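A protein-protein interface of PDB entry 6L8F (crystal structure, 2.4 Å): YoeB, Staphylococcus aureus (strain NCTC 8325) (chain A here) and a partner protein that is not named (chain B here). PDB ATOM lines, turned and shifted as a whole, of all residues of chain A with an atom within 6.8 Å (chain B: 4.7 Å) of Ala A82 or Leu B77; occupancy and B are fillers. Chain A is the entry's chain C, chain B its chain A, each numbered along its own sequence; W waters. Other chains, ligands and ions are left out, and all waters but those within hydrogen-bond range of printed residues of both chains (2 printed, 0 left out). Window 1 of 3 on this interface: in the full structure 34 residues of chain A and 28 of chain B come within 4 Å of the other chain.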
ATOM      1  N   THR A   7     -21.990   7.434 -18.784  1.00  0.00           N
ATOM      2  CA  THR A   7     -21.516   7.627 -17.418  1.00  0.00           C
ATOM      3  C   THR A   7     -22.713   7.787 -16.484  1.00  0.00           C
ATOM      4  O   THR A   7     -23.577   8.644 -16.714  1.00  0.00           O
ATOM      5  CB  THR A   7     -20.599   8.854 -17.333  1.00  0.00           C
ATOM      6  OG1 THR A   7     -19.381   8.588 -18.025  1.00  0.00           O
ATOM      7  CG2 THR A   7     -20.263   9.217 -15.887  1.00  0.00           C
ATOM      8  N   PHE A   8     -22.764   6.963 -15.438  1.00  0.00           N
ATOM      9  CA  PHE A   8     -23.843   6.978 -14.454  1.00  0.00           C
ATOM     10  C   PHE A   8     -23.365   7.543 -13.119  1.00  0.00           C
ATOM     11  O   PHE A   8     -22.253   7.249 -12.660  1.00  0.00           O
ATOM     12  CB  PHE A   8     -24.380   5.572 -14.171  1.00  0.00           C
ATOM     13  CG  PHE A   8     -25.100   4.927 -15.315  1.00  0.00           C
ATOM     14  CD1 PHE A   8     -24.398   4.287 -16.322  1.00  0.00           C
ATOM     15  CD2 PHE A   8     -26.482   4.889 -15.340  1.00  0.00           C
ATOM     16  CE1 PHE A   8     -25.059   3.668 -17.357  1.00  0.00           C
ATOM     17  CE2 PHE A   8     -27.141   4.273 -16.371  1.00  0.00           C
ATOM     18  CZ  PHE A   8     -26.428   3.661 -17.377  1.00  0.00           C
ATOM     19  N   SER A   9     -24.242   8.279 -12.454  1.00  0.00           N
ATOM     20  CA  SER A   9     -24.093   8.445 -11.020  1.00  0.00           C
ATOM     21  C   SER A   9     -24.342   7.089 -10.347  1.00  0.00           C
ATOM     22  O   SER A   9     -24.974   6.211 -10.944  1.00  0.00           O
ATOM     23  CB  SER A   9     -25.058   9.512 -10.516  1.00  0.00           C
ATOM     24  OG  SER A   9     -26.359   8.990 -10.364  1.00  0.00           O
ATOM     25  N   PRO A  10     -23.801   6.867  -9.131  1.00  0.00           N
ATOM     26  CA  PRO A  10     -23.977   5.543  -8.488  1.00  0.00           C
ATOM     27  C   PRO A  10     -25.427   5.159  -8.233  1.00  0.00           C
ATOM     28  O   PRO A  10     -25.813   4.005  -8.469  1.00  0.00           O
ATOM     29  CB  PRO A  10     -23.187   5.684  -7.178  1.00  0.00           C
ATOM     30  CG  PRO A  10     -22.138   6.690  -7.485  1.00  0.00           C
ATOM     31  CD  PRO A  10     -22.810   7.686  -8.410  1.00  0.00           C
ATOM     32  N   GLN A  11     -26.253   6.113  -7.809  1.00  0.00           N
ATOM     33  CA  GLN A  11     -27.662   5.821  -7.609  1.00  0.00           C
ATOM     34  C   GLN A  11     -28.387   5.613  -8.932  1.00  0.00           C
ATOM     35  O   GLN A  11     -29.310   4.796  -8.997  1.00  0.00           O
ATOM     36  CB  GLN A  11     -28.318   6.944  -6.802  1.00  0.00           C
ATOM     37  CG  GLN A  11     -27.727   7.120  -5.407  1.00  0.00           C
ATOM     38  CD  GLN A  11     -28.395   8.248  -4.623  1.00  0.00           C
ATOM     39  OE1 GLN A  11     -29.613   8.417  -4.670  1.00  0.00           O
ATOM     40  NE2 GLN A  11     -27.596   9.025  -3.903  1.00  0.00           N
ATOM     41  N   ALA A  12     -27.993   6.331  -9.991  1.00  0.00           N
ATOM     42  CA  ALA A  12     -28.636   6.116 -11.283  1.00  0.00           C
ATOM     43  C   ALA A  12     -28.299   4.746 -11.844  1.00  0.00           C
ATOM     44  O   ALA A  12     -29.139   4.133 -12.507  1.00  0.00           O
ATOM     45  CB  ALA A  12     -28.240   7.190 -12.295  1.00  0.00           C
ATOM     46  N   PHE A  13     -27.097   4.240 -11.559  1.00  0.00           N
ATOM     47  CA  PHE A  13     -26.715   2.929 -12.066  1.00  0.00           C
ATOM     48  C   PHE A  13     -27.432   1.815 -11.316  1.00  0.00           C
ATOM     49  O   PHE A  13     -27.836   0.820 -11.930  1.00  0.00           O
ATOM     50  CB  PHE A  13     -25.198   2.752 -11.977  1.00  0.00           C
ATOM     51  CG  PHE A  13     -24.702   1.489 -12.606  1.00  0.00           C
ATOM     52  CD1 PHE A  13     -24.740   1.326 -13.990  1.00  0.00           C
ATOM     53  CD2 PHE A  13     -24.188   0.462 -11.823  1.00  0.00           C
ATOM     54  CE1 PHE A  13     -24.277   0.148 -14.592  1.00  0.00           C
ATOM     55  CE2 PHE A  13     -23.717  -0.713 -12.415  1.00  0.00           C
ATOM     56  CZ  PHE A  13     -23.768  -0.869 -13.803  1.00  0.00           C
ATOM     57  N   ASP A  15     -30.431   2.051  -9.899  1.00  0.00           N
ATOM     58  CA  ASP A  15     -31.803   2.062 -10.396  1.00  0.00           C
ATOM     59  C   ASP A  15     -31.897   1.476 -11.802  1.00  0.00           C
ATOM     60  O   ASP A  15     -32.882   0.802 -12.130  1.00  0.00           O
ATOM     61  CB  ASP A  15     -32.352   3.488 -10.381  1.00  0.00           C
ATOM     62  CG  ASP A  15     -32.361   4.086  -8.993  1.00  0.00           C
ATOM     63  OD1 ASP A  15     -32.376   3.291  -8.030  1.00  0.00           O
ATOM     64  OD2 ASP A  15     -32.346   5.339  -8.868  1.00  0.00           O
ATOM     65  N   TYR A  59     -28.523  20.577 -16.346  1.00  0.00           N
ATOM     66  CA  TYR A  59     -29.078  19.263 -16.601  1.00  0.00           C
ATOM     67  C   TYR A  59     -30.420  19.407 -17.304  1.00  0.00           C
ATOM     68  O   TYR A  59     -30.995  20.500 -17.404  1.00  0.00           O
ATOM     69  CB  TYR A  59     -29.198  18.465 -15.291  1.00  0.00           C
ATOM     70  CG  TYR A  59     -27.867  17.892 -14.843  1.00  0.00           C
ATOM     71  CD1 TYR A  59     -26.908  18.699 -14.231  1.00  0.00           C
ATOM     72  CD2 TYR A  59     -27.556  16.549 -15.057  1.00  0.00           C
ATOM     73  CE1 TYR A  59     -25.679  18.187 -13.837  1.00  0.00           C
ATOM     74  CE2 TYR A  59     -26.326  16.026 -14.661  1.00  0.00           C
ATOM     75  CZ  TYR A  59     -25.397  16.853 -14.054  1.00  0.00           C
ATOM     76  OH  TYR A  59     -24.178  16.342 -13.662  1.00  0.00           O
ATOM     77  N   LEU A  70     -35.713  10.792 -16.808  1.00  0.00           N
ATOM     78  CA  LEU A  70     -34.290  10.646 -17.064  1.00  0.00           C
ATOM     79  C   LEU A  70     -33.654  12.019 -16.918  1.00  0.00           C
ATOM     80  O   LEU A  70     -33.981  12.936 -17.679  1.00  0.00           O
ATOM     81  CB  LEU A  70     -34.045  10.074 -18.456  1.00  0.00           C
ATOM     82  CG  LEU A  70     -32.583   9.893 -18.857  1.00  0.00           C
ATOM     83  CD1 LEU A  70     -31.986   8.678 -18.181  1.00  0.00           C
ATOM     84  CD2 LEU A  70     -32.472   9.795 -20.367  1.00  0.00           C
ATOM     85  N   VAL A  71     -32.772  12.177 -15.935  1.00  0.00           N
ATOM     86  CA  VAL A  71     -32.105  13.453 -15.687  1.00  0.00           C
ATOM     87  C   VAL A  71     -30.638  13.314 -16.067  1.00  0.00           C
ATOM     88  O   VAL A  71     -29.905  12.501 -15.486  1.00  0.00           O
ATOM     89  CB  VAL A  71     -32.253  13.922 -14.231  1.00  0.00           C
ATOM     90  CG1 VAL A  71     -31.571  15.276 -14.056  1.00  0.00           C
ATOM     91  CG2 VAL A  71     -33.732  13.986 -13.829  1.00  0.00           C
ATOM     92  N   TYR A  72     -30.202  14.144 -17.004  1.00  0.00           N
ATOM     93  CA  TYR A  72     -28.968  13.886 -17.714  1.00  0.00           C
ATOM     94  C   TYR A  72     -28.336  15.196 -18.136  1.00  0.00           C
ATOM     95  O   TYR A  72     -28.989  16.241 -18.195  1.00  0.00           O
ATOM     96  CB  TYR A  72     -29.192  13.008 -18.971  1.00  0.00           C
ATOM     97  CG  TYR A  72     -30.089  13.664 -20.003  1.00  0.00           C
ATOM     98  CD1 TYR A  72     -31.471  13.593 -19.881  1.00  0.00           C
ATOM     99  CD2 TYR A  72     -29.558  14.365 -21.092  1.00  0.00           C
ATOM    100  CE1 TYR A  72     -32.303  14.204 -20.795  1.00  0.00           C
ATOM    101  CE2 TYR A  72     -30.391  14.994 -22.010  1.00  0.00           C
ATOM    102  CZ  TYR A  72     -31.766  14.898 -21.860  1.00  0.00           C
ATOM    103  OH  TYR A  72     -32.613  15.499 -22.770  1.00  0.00           O
ATOM    104  N   THR A  73     -27.061  15.108 -18.489  1.00  0.00           N
ATOM    105  CA  THR A  73     -26.388  16.196 -19.169  1.00  0.00           C
ATOM    106  C   THR A  73     -25.495  15.585 -20.239  1.00  0.00           C
ATOM    107  O   THR A  73     -25.204  14.382 -20.225  1.00  0.00           O
ATOM    108  CB  THR A  73     -25.606  17.079 -18.178  1.00  0.00           C
ATOM    109  OG1 THR A  73     -25.260  18.317 -18.807  1.00  0.00           O
ATOM    110  CG2 THR A  73     -24.346  16.382 -17.689  1.00  0.00           C
ATOM    111  N   LYS A  80     -24.061  11.826 -19.560  1.00  0.00           N
ATOM    112  CA  LYS A  80     -23.953  11.559 -18.131  1.00  0.00           C
ATOM    113  C   LYS A  80     -25.359  11.473 -17.552  1.00  0.00           C
ATOM    114  O   LYS A  80     -26.188  12.332 -17.837  1.00  0.00           O
ATOM    115  CB  LYS A  80     -23.152  12.660 -17.426  1.00  0.00           C
ATOM    116  CG  LYS A  80     -21.765  12.903 -18.020  1.00  0.00           C
ATOM    117  CD  LYS A  80     -20.788  13.525 -17.006  1.00  0.00           C
ATOM    118  CE  LYS A  80     -21.110  14.974 -16.686  1.00  0.00           C
ATOM    119  NZ  LYS A  80     -20.002  15.692 -15.982  1.00  0.00           N
ATOM    120  N   ILE A  81     -25.638  10.450 -16.744  1.00  0.00           N
ATOM    121  CA  ILE A  81     -26.977  10.261 -16.184  1.00  0.00           C
ATOM    122  C   ILE A  81     -26.942  10.512 -14.682  1.00  0.00           C
ATOM    123  O   ILE A  81     -26.274   9.779 -13.942  1.00  0.00           O
ATOM    124  CB  ILE A  81     -27.535   8.861 -16.471  1.00  0.00           C
ATOM    125  CG1 ILE A  81     -27.629   8.620 -17.980  1.00  0.00           C
ATOM    126  CG2 ILE A  81     -28.918   8.701 -15.808  1.00  0.00           C
ATOM    127  CD1 ILE A  81     -28.349   7.323 -18.304  1.00  0.00           C
ATOM    128  N   ALA A  82     -27.691  11.526 -14.230  1.00  0.00           N
ATOM    129  CA  ALA A  82     -27.839  11.752 -12.794  1.00  0.00           C
ATOM    130  C   ALA A  82     -28.926  10.860 -12.208  1.00  0.00           C
ATOM    131  O   ALA A  82     -28.764  10.324 -11.107  1.00  0.00           O
ATOM    132  CB  ALA A  82     -28.144  13.230 -12.503  1.00  0.00           C
ATOM    133  N   SER A  83     -30.011  10.644 -12.952  1.00  0.00           N
ATOM    134  CA  SER A  83     -31.148   9.901 -12.435  1.00  0.00           C
ATOM    135  C   SER A  83     -31.891   9.209 -13.570  1.00  0.00           C
ATOM    136  O   SER A  83     -31.994   9.737 -14.681  1.00  0.00           O
ATOM    137  CB  SER A  83     -32.114  10.827 -11.690  1.00  0.00           C
ATOM    138  OG  SER A  83     -33.163  10.096 -11.088  1.00  0.00           O
ATOM    139  N   CYS A  84     -32.448   8.036 -13.266  1.00  0.00           N
ATOM    140  CA  CYS A  84     -33.432   7.431 -14.155  1.00  0.00           C
ATOM    141  C   CYS A  84     -34.638   6.886 -13.394  1.00  0.00           C
ATOM    142  O   CYS A  84     -35.341   6.012 -13.914  1.00  0.00           O
ATOM    143  CB  CYS A  84     -32.794   6.329 -15.001  1.00  0.00           C
ATOM    144  SG  CYS A  84     -32.152   4.949 -14.052  1.00  0.00           S
ATOM    145  N   HIS B  69     -31.491  13.070  -3.638  1.00  0.00           N
ATOM    146  CA  HIS B  69     -30.934  12.103  -4.578  1.00  0.00           C
ATOM    147  C   HIS B  69     -30.348  12.802  -5.796  1.00  0.00           C
ATOM    148  O   HIS B  69     -29.260  12.443  -6.258  1.00  0.00           O
ATOM    149  CB  HIS B  69     -32.021  11.098  -4.974  1.00  0.00           C
ATOM    150  CG  HIS B  69     -31.877  10.522  -6.351  1.00  0.00           C
ATOM    151  ND1 HIS B  69     -30.820   9.716  -6.718  1.00  0.00           N
ATOM    152  CD2 HIS B  69     -32.680  10.608  -7.438  1.00  0.00           C
ATOM    153  CE1 HIS B  69     -30.969   9.346  -7.980  1.00  0.00           C
ATOM    154  NE2 HIS B  69     -32.091   9.868  -8.438  1.00  0.00           N
ATOM    155  N   SER B  73     -26.347  12.918  -6.659  1.00  0.00           N
ATOM    156  CA  SER B  73     -25.946  12.331  -7.932  1.00  0.00           C
ATOM    157  C   SER B  73     -25.199  13.335  -8.792  1.00  0.00           C
ATOM    158  O   SER B  73     -24.207  12.981  -9.440  1.00  0.00           O
ATOM    159  CB  SER B  73     -27.172  11.812  -8.677  1.00  0.00           C
ATOM    160  OG  SER B  73     -27.718  10.694  -8.006  1.00  0.00           O
ATOM    161  N   ILE B  74     -25.674  14.584  -8.817  1.00  0.00           N
ATOM    162  CA  ILE B  74     -25.002  15.645  -9.560  1.00  0.00           C
ATOM    163  C   ILE B  74     -23.630  15.927  -8.960  1.00  0.00           C
ATOM    164  O   ILE B  74     -22.650  16.126  -9.689  1.00  0.00           O
ATOM    165  CB  ILE B  74     -25.903  16.892  -9.588  1.00  0.00           C
ATOM    166  CG1 ILE B  74     -27.013  16.691 -10.615  1.00  0.00           C
ATOM    167  CG2 ILE B  74     -25.122  18.177  -9.864  1.00  0.00           C
ATOM    168  CD1 ILE B  74     -28.146  17.681 -10.479  1.00  0.00           C
ATOM    169  N   ALA B  75     -23.535  15.880  -7.623  1.00  0.00           N
ATOM    170  CA  ALA B  75     -22.253  15.997  -6.932  1.00  0.00           C
ATOM    171  C   ALA B  75     -21.296  14.874  -7.317  1.00  0.00           C
ATOM    172  O   ALA B  75     -20.119  15.126  -7.597  1.00  0.00           O
ATOM    173  CB  ALA B  75     -22.479  15.992  -5.424  1.00  0.00           C
ATOM    174  N   ASP B  76     -21.784  13.628  -7.338  1.00  0.00           N
ATOM    175  CA  ASP B  76     -20.927  12.492  -7.676  1.00  0.00           C
ATOM    176  C   ASP B  76     -20.438  12.571  -9.120  1.00  0.00           C
ATOM    177  O   ASP B  76     -19.265  12.302  -9.394  1.00  0.00           O
ATOM    178  CB  ASP B  76     -21.675  11.185  -7.435  1.00  0.00           C
ATOM    179  CG  ASP B  76     -21.804  10.854  -5.961  1.00  0.00           C
ATOM    180  OD1 ASP B  76     -20.980  11.342  -5.163  1.00  0.00           O
ATOM    181  OD2 ASP B  76     -22.727  10.101  -5.603  1.00  0.00           O
ATOM    182  N   LEU B  77     -21.317  12.978 -10.038  1.00  0.00           N
ATOM    183  CA  LEU B  77     -20.906  13.271 -11.406  1.00  0.00           C
ATOM    184  C   LEU B  77     -19.836  14.355 -11.458  1.00  0.00           C
ATOM    185  O   LEU B  77     -18.887  14.254 -12.241  1.00  0.00           O
ATOM    186  CB  LEU B  77     -22.115  13.681 -12.238  1.00  0.00           C
ATOM    187  CG  LEU B  77     -23.041  12.525 -12.610  1.00  0.00           C
ATOM    188  CD1 LEU B  77     -24.346  13.068 -13.155  1.00  0.00           C
ATOM    189  CD2 LEU B  77     -22.379  11.640 -13.654  1.00  0.00           C
ATOM    190  N   GLU B  78     -19.939  15.379 -10.601  1.00  0.00           N
ATOM    191  CA  GLU B  78     -18.965  16.458 -10.688  1.00  0.00           C
ATOM    192  C   GLU B  78     -17.588  16.017 -10.192  1.00  0.00           C
ATOM    193  O   GLU B  78     -16.572  16.434 -10.757  1.00  0.00           O
ATOM    194  CB  GLU B  78     -19.462  17.697  -9.941  1.00  0.00           C
ATOM    195  CG  GLU B  78     -18.663  18.977 -10.269  1.00  0.00           C
ATOM    196  CD  GLU B  78     -17.427  19.104  -9.402  1.00  0.00           C
ATOM    197  OE1 GLU B  78     -17.441  18.463  -8.331  1.00  0.00           O
ATOM    198  OE2 GLU B  78     -16.445  19.760  -9.807  1.00  0.00           O
ATOM    199  N   ARG B  79     -17.512  15.198  -9.146  1.00  0.00           N
ATOM    200  CA  ARG B  79     -16.185  14.789  -8.712  1.00  0.00           C
ATOM    201  C   ARG B  79     -15.681  13.518  -9.390  1.00  0.00           C
ATOM    202  O   ARG B  79     -14.522  13.152  -9.176  1.00  0.00           O
ATOM    203  CB  ARG B  79     -16.131  14.609  -7.192  1.00  0.00           C
ATOM    204  CG  ARG B  79     -17.009  13.528  -6.644  1.00  0.00           C
ATOM    205  CD  ARG B  79     -16.714  13.331  -5.166  1.00  0.00           C
ATOM    206  NE  ARG B  79     -17.844  12.748  -4.447  1.00  0.00           N
ATOM    207  CZ  ARG B  79     -17.719  11.884  -3.441  1.00  0.00           C
ATOM    208  NH1 ARG B  79     -18.794  11.389  -2.834  1.00  0.00           N
ATOM    209  NH2 ARG B  79     -16.507  11.498  -3.056  1.00  0.00           N
ATOM    210  N   GLY B  80     -16.503  12.847 -10.194  1.00  0.00           N
ATOM    211  CA  GLY B  80     -16.085  11.649 -10.890  1.00  0.00           C
ATOM    212  C   GLY B  80     -16.272  10.346 -10.146  1.00  0.00           C
ATOM    213  O   GLY B  80     -15.693   9.331 -10.557  1.00  0.00           O
ATOM    214  N   THR B  82     -18.193   7.783 -10.250  1.00  0.00           N
ATOM    215  CA  THR B  82     -19.165   7.452 -11.279  1.00  0.00           C
ATOM    216  C   THR B  82     -18.915   6.041 -11.796  1.00  0.00           C
ATOM    217  O   THR B  82     -17.864   5.446 -11.561  1.00  0.00           O
ATOM    218  CB  THR B  82     -19.102   8.457 -12.444  1.00  0.00           C
ATOM    219  OG1 THR B  82     -17.760   8.545 -12.929  1.00  0.00           O
ATOM    220  CG2 THR B  82     -19.581   9.871 -12.030  1.00  0.00           C
HETATM  221  O   HOH W   1     -25.674   9.135  -7.140  1.00  0.00           O
HETATM  222  O   HOH W   2     -32.077   7.400 -10.540  1.00  0.00           O
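OG of Ser A9 lies within hydrogen-bond range of OG of Ser B73 (3.2 Å). The side-chain amide oxygen of Gln A11 is in hydrogen-bond range of a ring nitrogen (ND1) of His B69. O of Ala A82 sits close to OG of Ser B73, 3.3 Å away. A ring nitrogen (NE2) of His B69 sits at hydrogen-bond distance from the side-chain hydroxyl (OG) of Ser A83 (2.9 Å).
O of Thr A7 is in hydrogen-bond range of N of Ile A81. The backbone carbonyl oxygen (O) of Ala A82 lies within hydrogen-bond range of the side-chain hydroxyl (OG) of Ser A9 (2.8 Å). The backbone NH of Val A71 sits at hydrogen-bond distance from the backbone carbonyl oxygen of Ser A83 (2.9 Å). The backbone carbonyl oxygen (O) of Thr A73 lies within hydrogen-bond range of the backbone NH (N) of Lys A80 (2.9 Å). The side-chain carboxylate (OD1) of Asp B76 is in salt-bridge range of the guanidinium group (NH1) of Arg B79 (3.2 Å). OG1 of Thr B82 lies within hydrogen-bond range of O of Gly B80, at 3.2 Å.
CG2 of Thr A7 touches CD2 of Leu B77 (3.9 Å). CB of Thr B82 touches CG2 of Thr A7, at 3.7 Å. O of Phe A8 touches CB of Thr B82, 3.4 Å away. Pro A10 touches Asp B76 (CD to OD2, 3.7 Å). CB of Gln A11 touches OG of Ser B73 (3.98 Å). Ile B74 touches Tyr A59. CD2 of Leu B77 touches CB of Lys A80, at 3.98 Å. O of Ile A81 touches CD1 of Leu B77 (3.9 Å). O of Ala A82 touches CE1 of His B69 (3.9 Å). Leu B77 touches Ala A82.
Printed residues of chain B within 4 Å of Tyr A59: Ile B74 and Leu B77. Tyr A72 touches none of the printed residues of chain B. Of the printed residues of chain A, His B69 touches Gln A11 (2.7 Å), Ala A82 (3.9 Å) and Ser A83 (2.9 Å). Of the printed residues of chain A, Leu B77 touches Thr A7, Tyr A59, Lys A80, Ile A81 and Ala A82. The nearest residue of chain B that does not touch Ala A82 is Ile B74 (4.1 Å). The nearest printed residue of chain B that does not touch Ser A83 is Ser B73 (5.3 Å).
Printed residues of chain A that touch a printed residue of chain B: Thr A7, Phe A8, Ser A9, Pro A10, Gln A11, Tyr A59, Lys A80, Ile A81, Ala A82 and Ser A83. Of the 10 printed residues of chain B, 6 touch a printed residue of chain A. Along chain B the printed residues that touch a printed residue of chain A span positions 69 to 82. Among the printed residues, 15 pairs touch across the chains.
Water W2 lies within hydrogen-bond range of OD2 of Asp A15 (2.7 Å), N of Cys A84 (2.8 Å), OG of Ser A83 (3.0 Å) and NE2 of His B69 (3.2 Å). Water W1 lies within hydrogen-bond range of the side-chain hydroxyl (OG) of Ser B73 (2.7 Å), the backbone NH (N) of Gln A11 (3.1 Å), the side-chain hydroxyl (OG) of Ser A9 (3.3 Å) and the side-chain carboxylate (OD2) of Asp B76 (3.5 Å).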
